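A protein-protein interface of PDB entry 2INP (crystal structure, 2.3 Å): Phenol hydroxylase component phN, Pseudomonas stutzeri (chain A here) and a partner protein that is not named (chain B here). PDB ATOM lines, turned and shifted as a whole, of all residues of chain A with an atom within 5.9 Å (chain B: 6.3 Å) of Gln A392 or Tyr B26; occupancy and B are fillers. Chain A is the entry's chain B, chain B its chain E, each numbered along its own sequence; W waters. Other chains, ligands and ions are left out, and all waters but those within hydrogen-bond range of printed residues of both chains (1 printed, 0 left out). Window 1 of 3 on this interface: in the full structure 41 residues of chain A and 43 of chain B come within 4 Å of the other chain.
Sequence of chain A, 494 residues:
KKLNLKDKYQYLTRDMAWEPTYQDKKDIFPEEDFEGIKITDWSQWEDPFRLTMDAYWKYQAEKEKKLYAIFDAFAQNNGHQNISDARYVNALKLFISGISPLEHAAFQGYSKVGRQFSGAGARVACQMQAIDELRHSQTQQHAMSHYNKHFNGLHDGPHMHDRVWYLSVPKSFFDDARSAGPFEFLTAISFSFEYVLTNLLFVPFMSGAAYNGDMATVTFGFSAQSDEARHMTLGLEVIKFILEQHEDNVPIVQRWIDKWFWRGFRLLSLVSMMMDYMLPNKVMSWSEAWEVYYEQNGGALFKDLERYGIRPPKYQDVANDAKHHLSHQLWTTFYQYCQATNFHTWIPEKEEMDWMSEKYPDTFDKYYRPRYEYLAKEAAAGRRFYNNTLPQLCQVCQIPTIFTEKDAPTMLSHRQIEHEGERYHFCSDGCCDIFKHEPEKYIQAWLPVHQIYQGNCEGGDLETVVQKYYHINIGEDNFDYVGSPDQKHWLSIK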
ATOM      1  N   LEU A 390      -8.811 -10.057   9.973  1.00  0.00           N
ATOM      2  CA  LEU A 390      -7.996  -9.600  11.101  1.00  0.00           C
ATOM      3  C   LEU A 390      -7.965  -8.093  11.208  1.00  0.00           C
ATOM      4  O   LEU A 390      -8.230  -7.403  10.226  1.00  0.00           O
ATOM      5  CB  LEU A 390      -6.568 -10.100  10.940  1.00  0.00           C
ATOM      6  CG  LEU A 390      -6.243 -11.620  11.021  1.00  0.00           C
ATOM      7  CD1 LEU A 390      -4.803 -11.869  10.489  1.00  0.00           C
ATOM      8  CD2 LEU A 390      -6.393 -12.121  12.487  1.00  0.00           C
ATOM      9  N   PRO A 391      -7.702  -7.582  12.437  1.00  0.00           N
ATOM     10  CA  PRO A 391      -7.846  -6.190  12.738  1.00  0.00           C
ATOM     11  C   PRO A 391      -6.560  -5.447  12.622  1.00  0.00           C
ATOM     12  O   PRO A 391      -5.488  -6.065  12.736  1.00  0.00           O
ATOM     13  CB  PRO A 391      -8.242  -6.213  14.258  1.00  0.00           C
ATOM     14  CG  PRO A 391      -7.349  -7.310  14.814  1.00  0.00           C
ATOM     15  CD  PRO A 391      -7.420  -8.389  13.665  1.00  0.00           C
ATOM     16  N   GLN A 392      -6.673  -4.121  12.429  1.00  0.00           N
ATOM     17  CA  GLN A 392      -5.601  -3.216  12.678  1.00  0.00           C
ATOM     18  C   GLN A 392      -5.262  -3.270  14.175  1.00  0.00           C
ATOM     19  O   GLN A 392      -6.203  -3.285  15.001  1.00  0.00           O
ATOM     20  CB  GLN A 392      -6.088  -1.807  12.312  1.00  0.00           C
ATOM     21  CG  GLN A 392      -5.099  -0.701  12.563  1.00  0.00           C
ATOM     22  CD  GLN A 392      -5.679   0.684  12.231  1.00  0.00           C
ATOM     23  OE1 GLN A 392      -6.440   1.214  13.028  1.00  0.00           O
ATOM     24  NE2 GLN A 392      -5.320   1.269  11.030  1.00  0.00           N
ATOM     25  N   LEU A 393      -3.954  -3.249  14.512  1.00  0.00           N
ATOM     26  CA  LEU A 393      -3.463  -3.318  15.866  1.00  0.00           C
ATOM     27  C   LEU A 393      -2.802  -2.000  16.167  1.00  0.00           C
ATOM     28  O   LEU A 393      -2.124  -1.399  15.297  1.00  0.00           O
ATOM     29  CB  LEU A 393      -2.346  -4.409  16.025  1.00  0.00           C
ATOM     30  CG  LEU A 393      -2.804  -5.880  15.925  1.00  0.00           C
ATOM     31  CD1 LEU A 393      -1.663  -6.742  16.240  1.00  0.00           C
ATOM     32  CD2 LEU A 393      -3.962  -6.157  16.865  1.00  0.00           C
ATOM     33  N   CYS A 394      -2.900  -1.574  17.405  1.00  0.00           N
ATOM     34  CA  CYS A 394      -2.104  -0.466  17.816  1.00  0.00           C
ATOM     35  C   CYS A 394      -0.574  -0.748  17.856  1.00  0.00           C
ATOM     36  O   CYS A 394      -0.105  -1.713  18.470  1.00  0.00           O
ATOM     37  CB  CYS A 394      -2.588   0.024  19.191  1.00  0.00           C
ATOM     38  SG  CYS A 394      -1.612   1.521  19.758  1.00  0.00           S
ATOM     39  N   ILE A 399      -3.144  -3.684  21.057  1.00  0.00           N
ATOM     40  CA  ILE A 399      -4.563  -4.122  21.136  1.00  0.00           C
ATOM     41  C   ILE A 399      -5.154  -3.671  19.795  1.00  0.00           C
ATOM     42  O   ILE A 399      -4.712  -2.621  19.274  1.00  0.00           O
ATOM     43  CB  ILE A 399      -5.306  -3.421  22.319  1.00  0.00           C
ATOM     44  CG1 ILE A 399      -4.663  -3.793  23.686  1.00  0.00           C
ATOM     45  CG2 ILE A 399      -6.774  -3.750  22.324  1.00  0.00           C
ATOM     46  CD1 ILE A 399      -5.238  -3.051  24.827  1.00  0.00           C
ATOM     47  N   PRO A 400      -6.114  -4.444  19.216  1.00  0.00           N
ATOM     48  CA  PRO A 400      -6.755  -3.886  18.058  1.00  0.00           C
ATOM     49  C   PRO A 400      -7.302  -2.469  18.305  1.00  0.00           C
ATOM     50  O   PRO A 400      -7.645  -2.106  19.475  1.00  0.00           O
ATOM     51  CB  PRO A 400      -7.877  -4.896  17.756  1.00  0.00           C
ATOM     52  CG  PRO A 400      -7.900  -5.809  18.814  1.00  0.00           C
ATOM     53  CD  PRO A 400      -6.612  -5.796  19.490  1.00  0.00           C
ATOM     54  N   THR A 401      -7.405  -1.677  17.233  1.00  0.00           N
ATOM     55  CA  THR A 401      -7.830  -0.267  17.350  1.00  0.00           C
ATOM     56  C   THR A 401      -9.384  -0.143  17.509  1.00  0.00           C
ATOM     57  O   THR A 401     -10.142   0.386  16.629  1.00  0.00           O
ATOM     58  CB  THR A 401      -7.284   0.541  16.162  1.00  0.00           C
ATOM     59  OG1 THR A 401      -7.491  -0.222  14.955  1.00  0.00           O
ATOM     60  CG2 THR A 401      -5.805   0.884  16.352  1.00  0.00           C
ATOM     61  N   ILE A 402      -9.868  -0.618  18.668  1.00  0.00           N
ATOM     62  CA  ILE A 402     -11.285  -0.754  18.926  1.00  0.00           C
ATOM     63  C   ILE A 402     -11.784   0.377  19.836  1.00  0.00           C
ATOM     64  O   ILE A 402     -12.987   0.449  20.108  1.00  0.00           O
ATOM     65  CB  ILE A 402     -11.528  -2.045  19.653  1.00  0.00           C
ATOM     66  CG1 ILE A 402     -10.885  -1.932  21.080  1.00  0.00           C
ATOM     67  CG2 ILE A 402     -11.019  -3.166  18.781  1.00  0.00           C
ATOM     68  CD1 ILE A 402     -11.141  -3.079  21.954  1.00  0.00           C
ATOM     69  N   HIS A 414      -8.769   6.248  16.297  1.00  0.00           N
ATOM     70  CA  HIS A 414      -7.633   6.028  15.411  1.00  0.00           C
ATOM     71  C   HIS A 414      -6.746   7.241  15.351  1.00  0.00           C
ATOM     72  O   HIS A 414      -7.279   8.328  15.166  1.00  0.00           O
ATOM     73  CB  HIS A 414      -8.071   5.729  13.959  1.00  0.00           C
ATOM     74  CG  HIS A 414      -6.899   5.502  13.061  1.00  0.00           C
ATOM     75  ND1 HIS A 414      -6.361   6.495  12.268  1.00  0.00           N
ATOM     76  CD2 HIS A 414      -6.083   4.422  12.913  1.00  0.00           C
ATOM     77  CE1 HIS A 414      -5.304   6.023  11.626  1.00  0.00           C
ATOM     78  NE2 HIS A 414      -5.109   4.770  12.002  1.00  0.00           N
ATOM     79  N   HIS A 425       0.183   3.347  13.076  1.00  0.00           N
ATOM     80  CA  HIS A 425      -1.171   3.589  13.496  1.00  0.00           C
ATOM     81  C   HIS A 425      -1.296   3.316  15.025  1.00  0.00           C
ATOM     82  O   HIS A 425      -0.546   2.479  15.587  1.00  0.00           O
ATOM     83  CB  HIS A 425      -2.109   2.706  12.697  1.00  0.00           C
ATOM     84  CG  HIS A 425      -2.056   2.934  11.202  1.00  0.00           C
ATOM     85  ND1 HIS A 425      -3.000   3.684  10.526  1.00  0.00           N
ATOM     86  CD2 HIS A 425      -1.200   2.477  10.248  1.00  0.00           C
ATOM     87  CE1 HIS A 425      -2.699   3.728   9.234  1.00  0.00           C
ATOM     88  NE2 HIS A 425      -1.597   3.016   9.046  1.00  0.00           N
ATOM     89  N   PHE A 426      -2.205   4.035  15.700  1.00  0.00           N
ATOM     90  CA  PHE A 426      -2.373   3.935  17.152  1.00  0.00           C
ATOM     91  C   PHE A 426      -3.851   3.928  17.519  1.00  0.00           C
ATOM     92  O   PHE A 426      -4.697   4.420  16.713  1.00  0.00           O
ATOM     93  CB  PHE A 426      -1.677   5.060  17.855  1.00  0.00           C
ATOM     94  CG  PHE A 426      -0.292   5.332  17.319  1.00  0.00           C
ATOM     95  CD1 PHE A 426       0.809   4.642  17.823  1.00  0.00           C
ATOM     96  CD2 PHE A 426      -0.109   6.202  16.238  1.00  0.00           C
ATOM     97  CE1 PHE A 426       2.066   4.838  17.265  1.00  0.00           C
ATOM     98  CE2 PHE A 426       1.180   6.431  15.686  1.00  0.00           C
ATOM     99  CZ  PHE A 426       2.244   5.768  16.201  1.00  0.00           C
ATOM    100  N   LEU A 447       4.214  -7.460  15.748  1.00  0.00           N
ATOM    101  CA  LEU A 447       2.773  -7.296  15.750  1.00  0.00           C
ATOM    102  C   LEU A 447       2.127  -8.528  15.160  1.00  0.00           C
ATOM    103  O   LEU A 447       2.278  -8.815  13.979  1.00  0.00           O
ATOM    104  CB  LEU A 447       2.283  -6.052  14.978  1.00  0.00           C
ATOM    105  CG  LEU A 447       2.561  -4.580  15.342  1.00  0.00           C
ATOM    106  CD1 LEU A 447       1.484  -3.559  14.686  1.00  0.00           C
ATOM    107  CD2 LEU A 447       2.668  -4.324  16.825  1.00  0.00           C
ATOM    108  N   VAL A 449      -0.590  -9.764  13.895  1.00  0.00           N
ATOM    109  CA  VAL A 449      -1.373  -9.737  12.624  1.00  0.00           C
ATOM    110  C   VAL A 449      -0.407  -9.536  11.430  1.00  0.00           C
ATOM    111  O   VAL A 449      -0.522 -10.209  10.419  1.00  0.00           O
ATOM    112  CB  VAL A 449      -2.483  -8.651  12.637  1.00  0.00           C
ATOM    113  CG1 VAL A 449      -3.117  -8.410  11.222  1.00  0.00           C
ATOM    114  CG2 VAL A 449      -3.645  -8.968  13.634  1.00  0.00           C
ATOM    115  N   HIS A 450       0.564  -8.641  11.590  1.00  0.00           N
ATOM    116  CA  HIS A 450       1.529  -8.348  10.552  1.00  0.00           C
ATOM    117  C   HIS A 450       2.413  -9.531  10.317  1.00  0.00           C
ATOM    118  O   HIS A 450       2.744  -9.808   9.165  1.00  0.00           O
ATOM    119  CB  HIS A 450       2.389  -7.191  10.953  1.00  0.00           C
ATOM    120  CG  HIS A 450       1.658  -5.886  11.040  1.00  0.00           C
ATOM    121  ND1 HIS A 450       0.316  -5.750  10.722  1.00  0.00           N
ATOM    122  CD2 HIS A 450       2.096  -4.647  11.342  1.00  0.00           C
ATOM    123  CE1 HIS A 450      -0.052  -4.489  10.879  1.00  0.00           C
ATOM    124  NE2 HIS A 450       1.002  -3.806  11.297  1.00  0.00           N
ATOM    125  N   LEU B  24       0.344  -4.134   3.138  1.00  0.00           N
ATOM    126  CA  LEU B  24      -0.768  -3.891   4.069  1.00  0.00           C
ATOM    127  C   LEU B  24      -1.715  -2.750   3.670  1.00  0.00           C
ATOM    128  O   LEU B  24      -1.270  -1.624   3.324  1.00  0.00           O
ATOM    129  CB  LEU B  24      -0.272  -3.625   5.442  1.00  0.00           C
ATOM    130  CG  LEU B  24       0.178  -4.862   6.261  1.00  0.00           C
ATOM    131  CD1 LEU B  24       0.931  -4.379   7.459  1.00  0.00           C
ATOM    132  CD2 LEU B  24      -1.042  -5.753   6.671  1.00  0.00           C
ATOM    133  N   LEU B  25      -3.009  -2.993   3.785  1.00  0.00           N
ATOM    134  CA  LEU B  25      -4.000  -1.868   3.680  1.00  0.00           C
ATOM    135  C   LEU B  25      -4.995  -1.938   4.842  1.00  0.00           C
ATOM    136  O   LEU B  25      -5.558  -3.019   5.109  1.00  0.00           O
ATOM    137  CB  LEU B  25      -4.830  -2.024   2.362  1.00  0.00           C
ATOM    138  CG  LEU B  25      -5.958  -1.013   2.052  1.00  0.00           C
ATOM    139  CD1 LEU B  25      -5.405   0.401   2.088  1.00  0.00           C
ATOM    140  CD2 LEU B  25      -6.502  -1.274   0.732  1.00  0.00           C
ATOM    141  N   TYR B  26      -5.254  -0.838   5.533  1.00  0.00           N
ATOM    142  CA  TYR B  26      -6.358  -0.771   6.516  1.00  0.00           C
ATOM    143  C   TYR B  26      -7.566  -0.098   5.874  1.00  0.00           C
ATOM    144  O   TYR B  26      -7.414   0.755   4.997  1.00  0.00           O
ATOM    145  CB  TYR B  26      -5.917   0.002   7.751  1.00  0.00           C
ATOM    146  CG  TYR B  26      -4.637  -0.518   8.320  1.00  0.00           C
ATOM    147  CD1 TYR B  26      -3.480   0.211   8.172  1.00  0.00           C
ATOM    148  CD2 TYR B  26      -4.582  -1.811   8.944  1.00  0.00           C
ATOM    149  CE1 TYR B  26      -2.232  -0.235   8.672  1.00  0.00           C
ATOM    150  CE2 TYR B  26      -3.341  -2.331   9.445  1.00  0.00           C
ATOM    151  CZ  TYR B  26      -2.166  -1.529   9.314  1.00  0.00           C
ATOM    152  OH  TYR B  26      -0.934  -1.966   9.771  1.00  0.00           O
ATOM    153  N   VAL B  27      -8.766  -0.522   6.262  1.00  0.00           N
ATOM    154  CA  VAL B  27      -9.971   0.106   5.784  1.00  0.00           C
ATOM    155  C   VAL B  27     -10.814   0.312   7.075  1.00  0.00           C
ATOM    156  O   VAL B  27     -11.014  -0.633   7.829  1.00  0.00           O
ATOM    157  CB  VAL B  27     -10.721  -0.734   4.681  1.00  0.00           C
ATOM    158  CG1 VAL B  27     -12.059  -0.026   4.194  1.00  0.00           C
ATOM    159  CG2 VAL B  27      -9.846  -0.995   3.513  1.00  0.00           C
ATOM    160  N   TYR B  28     -11.263   1.555   7.327  1.00  0.00           N
ATOM    161  CA  TYR B  28     -12.260   1.908   8.338  1.00  0.00           C
ATOM    162  C   TYR B  28     -13.591   2.264   7.679  1.00  0.00           C
ATOM    163  O   TYR B  28     -13.615   3.120   6.811  1.00  0.00           O
ATOM    164  CB  TYR B  28     -11.723   3.052   9.129  1.00  0.00           C
ATOM    165  CG  TYR B  28     -12.624   3.608  10.236  1.00  0.00           C
ATOM    166  CD1 TYR B  28     -12.509   4.966  10.637  1.00  0.00           C
ATOM    167  CD2 TYR B  28     -13.529   2.776  10.921  1.00  0.00           C
ATOM    168  CE1 TYR B  28     -13.322   5.501  11.711  1.00  0.00           C
ATOM    169  CE2 TYR B  28     -14.332   3.296  11.949  1.00  0.00           C
ATOM    170  CZ  TYR B  28     -14.214   4.635  12.353  1.00  0.00           C
ATOM    171  OH  TYR B  28     -15.057   5.090  13.321  1.00  0.00           O
ATOM    172  N   ALA B  37     -12.785  -3.110  14.659  1.00  0.00           N
ATOM    173  CA  ALA B  37     -11.591  -2.272  14.384  1.00  0.00           C
ATOM    174  C   ALA B  37     -11.542  -2.230  12.862  1.00  0.00           C
ATOM    175  O   ALA B  37     -12.087  -3.189  12.197  1.00  0.00           O
ATOM    176  CB  ALA B  37     -10.334  -2.961  14.930  1.00  0.00           C
ATOM    177  N   PRO B  38     -10.830  -1.203  12.285  1.00  0.00           N
ATOM    178  CA  PRO B  38     -10.530  -1.258  10.864  1.00  0.00           C
ATOM    179  C   PRO B  38      -9.859  -2.603  10.502  1.00  0.00           C
ATOM    180  O   PRO B  38      -8.973  -3.080  11.238  1.00  0.00           O
ATOM    181  CB  PRO B  38      -9.494  -0.146  10.676  1.00  0.00           C
ATOM    182  CG  PRO B  38      -9.841   0.787  11.701  1.00  0.00           C
ATOM    183  CD  PRO B  38     -10.181  -0.039  12.902  1.00  0.00           C
ATOM    184  N   PHE B  39     -10.249  -3.147   9.370  1.00  0.00           N
ATOM    185  CA  PHE B  39      -9.651  -4.311   8.759  1.00  0.00           C
ATOM    186  C   PHE B  39      -8.221  -4.072   8.439  1.00  0.00           C
ATOM    187  O   PHE B  39      -7.857  -2.977   7.975  1.00  0.00           O
ATOM    188  CB  PHE B  39     -10.369  -4.653   7.449  1.00  0.00           C
ATOM    189  CG  PHE B  39     -11.832  -4.931   7.632  1.00  0.00           C
ATOM    190  CD1 PHE B  39     -12.790  -4.331   6.791  1.00  0.00           C
ATOM    191  CD2 PHE B  39     -12.277  -5.792   8.648  1.00  0.00           C
ATOM    192  CE1 PHE B  39     -14.119  -4.587   6.962  1.00  0.00           C
ATOM    193  CE2 PHE B  39     -13.653  -6.043   8.789  1.00  0.00           C
ATOM    194  CZ  PHE B  39     -14.543  -5.418   7.956  1.00  0.00           C
ATOM    195  N   ALA B  40      -7.441  -5.111   8.650  1.00  0.00           N
ATOM    196  CA  ALA B  40      -6.068  -5.220   8.234  1.00  0.00           C
ATOM    197  C   ALA B  40      -6.079  -6.234   7.077  1.00  0.00           C
ATOM    198  O   ALA B  40      -6.394  -7.456   7.262  1.00  0.00           O
ATOM    199  CB  ALA B  40      -5.250  -5.716   9.371  1.00  0.00           C
ATOM    200  N   LEU B  41      -5.778  -5.716   5.882  1.00  0.00           N
ATOM    201  CA  LEU B  41      -5.934  -6.430   4.605  1.00  0.00           C
ATOM    202  C   LEU B  41      -4.561  -6.566   4.036  1.00  0.00           C
ATOM    203  O   LEU B  41      -3.752  -5.659   4.181  1.00  0.00           O
ATOM    204  CB  LEU B  41      -6.812  -5.623   3.619  1.00  0.00           C
ATOM    205  CG  LEU B  41      -8.279  -5.306   4.019  1.00  0.00           C
ATOM    206  CD1 LEU B  41      -9.030  -4.484   2.911  1.00  0.00           C
ATOM    207  CD2 LEU B  41      -9.086  -6.605   4.328  1.00  0.00           C
ATOM    208  N   HIS B  99       1.870   1.084   1.367  1.00  0.00           N
ATOM    209  CA  HIS B  99       1.874   0.082   2.388  1.00  0.00           C
ATOM    210  C   HIS B  99       1.465   0.752   3.697  1.00  0.00           C
ATOM    211  O   HIS B  99       2.036   1.767   4.101  1.00  0.00           O
ATOM    212  CB  HIS B  99       3.250  -0.535   2.427  1.00  0.00           C
ATOM    213  CG  HIS B  99       3.472  -1.553   3.519  1.00  0.00           C
ATOM    214  ND1 HIS B  99       2.737  -2.713   3.634  1.00  0.00           N
ATOM    215  CD2 HIS B  99       4.386  -1.592   4.513  1.00  0.00           C
ATOM    216  CE1 HIS B  99       3.239  -3.453   4.601  1.00  0.00           C
ATOM    217  NE2 HIS B  99       4.244  -2.800   5.156  1.00  0.00           N
ATOM    218  N   LYS B 100       0.495   0.105   4.351  1.00  0.00           N
ATOM    219  CA  LYS B 100      -0.045   0.516   5.620  1.00  0.00           C
ATOM    220  C   LYS B 100      -0.739   1.858   5.522  1.00  0.00           C
ATOM    221  O   LYS B 100      -0.844   2.559   6.513  1.00  0.00           O
ATOM    222  CB  LYS B 100       1.010   0.563   6.725  1.00  0.00           C
ATOM    223  CG  LYS B 100       1.528  -0.840   7.154  1.00  0.00           C
ATOM    224  CD  LYS B 100       2.333  -0.752   8.453  1.00  0.00           C
ATOM    225  CE  LYS B 100       3.793  -0.368   8.243  1.00  0.00           C
ATOM    226  NZ  LYS B 100       4.416   0.061   9.571  1.00  0.00           N
ATOM    227  N   SER B 101      -1.197   2.229   4.319  1.00  0.00           N
ATOM    228  CA  SER B 101      -2.138   3.334   4.236  1.00  0.00           C
ATOM    229  C   SER B 101      -3.419   2.844   4.903  1.00  0.00           C
ATOM    230  O   SER B 101      -3.687   1.634   4.932  1.00  0.00           O
ATOM    231  CB  SER B 101      -2.444   3.640   2.765  1.00  0.00           C
ATOM    232  OG  SER B 101      -1.323   4.275   2.131  1.00  0.00           O
ATOM    233  N   MET B 102      -4.249   3.785   5.364  1.00  0.00           N
ATOM    234  CA  MET B 102      -5.634   3.513   5.724  1.00  0.00           C
ATOM    235  C   MET B 102      -6.635   4.313   4.830  1.00  0.00           C
ATOM    236  O   MET B 102      -6.585   5.564   4.733  1.00  0.00           O
ATOM    237  CB  MET B 102      -5.852   3.832   7.222  1.00  0.00           C
ATOM    238  CG  MET B 102      -7.308   3.542   7.686  1.00  0.00           C
ATOM    239  SD  MET B 102      -7.582   3.195   9.434  1.00  0.00           S
ATOM    240  CE  MET B 102      -8.494   4.725   9.878  1.00  0.00           C
ATOM    241  N   LEU B 103      -7.539   3.578   4.210  1.00  0.00           N
ATOM    242  CA  LEU B 103      -8.717   4.116   3.623  1.00  0.00           C
ATOM    243  C   LEU B 103      -9.867   4.125   4.626  1.00  0.00           C
ATOM    244  O   LEU B 103     -10.084   3.135   5.339  1.00  0.00           O
ATOM    245  CB  LEU B 103      -9.109   3.299   2.363  1.00  0.00           C
ATOM    246  CG  LEU B 103      -8.159   3.302   1.155  1.00  0.00           C
ATOM    247  CD1 LEU B 103      -8.514   2.141   0.363  1.00  0.00           C
ATOM    248  CD2 LEU B 103      -8.344   4.578   0.325  1.00  0.00           C
ATOM    249  N   THR B 104     -10.625   5.226   4.675  1.00  0.00           N
ATOM    250  CA  THR B 104     -11.889   5.337   5.451  1.00  0.00           C
ATOM    251  C   THR B 104     -13.004   5.451   4.391  1.00  0.00           C
ATOM    252  O   THR B 104     -12.931   6.322   3.510  1.00  0.00           O
ATOM    253  CB  THR B 104     -11.917   6.623   6.307  1.00  0.00           C
ATOM    254  OG1 THR B 104     -10.665   6.794   7.017  1.00  0.00           O
ATOM    255  CG2 THR B 104     -13.095   6.655   7.261  1.00  0.00           C
HETATM  256  O   HOH W   1      -1.038  -0.881  12.767  1.00  0.00           O
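Water W1 bridges O of Leu A393 (2.8 Å) and OH of Tyr B26 (3.2 Å).
Of chain B, only Tyr B26 (3.3 Å), Pro B38 (2.8 Å), Ala B40 (3.7 Å) and Met B102 (3.4 Å) come within 4 Å of Gln A392.
Of the printed residues of chain A, Tyr B26 touches Gln A392, His A425 and His A450.
Of the printed residues of chain A, Met B102 touches Gln A392 (3.4 Å), His A414 (3.6 Å) and His A425 (3.7 Å).
Of the printed residues of chain A, Ala B40 touches Leu A390 (2.9 Å), Pro A391 (3.4 Å), Gln A392 (3.7 Å) and Val A449 (3.9 Å).
The nearest residue of chain B that does not touch Gln A392 is Ala B37 (4.1 Å).
The nearest residue of chain A that does not touch Tyr B26 is Leu A393 (5.2 Å).
The nearest printed residue of chain B that does not touch His A414 is Pro B38 (5.4 Å).
Printed residues of chain A that touch a printed residue of chain B: Leu A390, Pro A391, Gln A392, Thr A401, Ile A402, His A414, His A425, Val A449 and His A450.
Hydrophobic or aromatic side chains of chain B that line the printed part of chain A: Leu B24, Tyr B26, Ala B37, Pro B38, Ala B40 and Met B102.
Among the printed residues, no Asp or Glu carboxylate lies within 4 Å of a Lys or Arg side-chain nitrogen of the other chain.
N of Leu B103 sits at hydrogen-bond distance from O of Tyr B26 (2.9 Å).
A ring nitrogen (ND1) of His A425 lies within hydrogen-bond range of a ring nitrogen (NE2) of His A414 (2.8 Å).
The backbone NH (N) of Tyr B26 lies within hydrogen-bond range of the backbone carbonyl oxygen (O) of Ser B101.
The backbone carbonyl oxygen of Val B27 is in hydrogen-bond range of the backbone NH of Phe B39.
The backbone NH (N) of Leu B24 sits at hydrogen-bond distance from a ring nitrogen (ND1) of His B99, at 2.8 Å.
The side-chain amide nitrogen of Gln A392 is in hydrogen-bond range of a ring nitrogen (ND1) of His A425 (3.4 Å).
O of Leu A390 touches CA of Phe B39, 3.7 Å away.
Pro A391 touches Ala B37.
Gln A392 touches Tyr B26 (NE2 to CG, 3.3 Å).
Gln A392 touches Ala B40 (N to CB, 3.7 Å).
Ala B37 touches Thr A401.
CG2 of Ile A402 touches CB of Ala B37, at 3.9 Å.
His A414 touches Met B102.
Tyr B26 touches His A425 (CE1 to CD2, 3.3 Å).
Met B102 touches His A425.
His A450 touches Leu B24.
NE2 of His A425 is in hydrogen-bond range of O of Lys B100, at 2.7 Å.
The side-chain sulfur of Met B102 lies within hydrogen-bond range of the side-chain amide nitrogen of Gln A392 (3.4 Å).
The backbone carbonyl oxygen (O) of Pro B38 lies within hydrogen-bond range of the backbone NH (N) of Gln A392 (2.8 Å).
A ring nitrogen (NE2) of His A450 sits close to the side-chain hydroxyl (OH) of Tyr B26, 3.1 Å away.
N of Ala B40 is in hydrogen-bond range of O of Leu A390 (2.9 Å).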
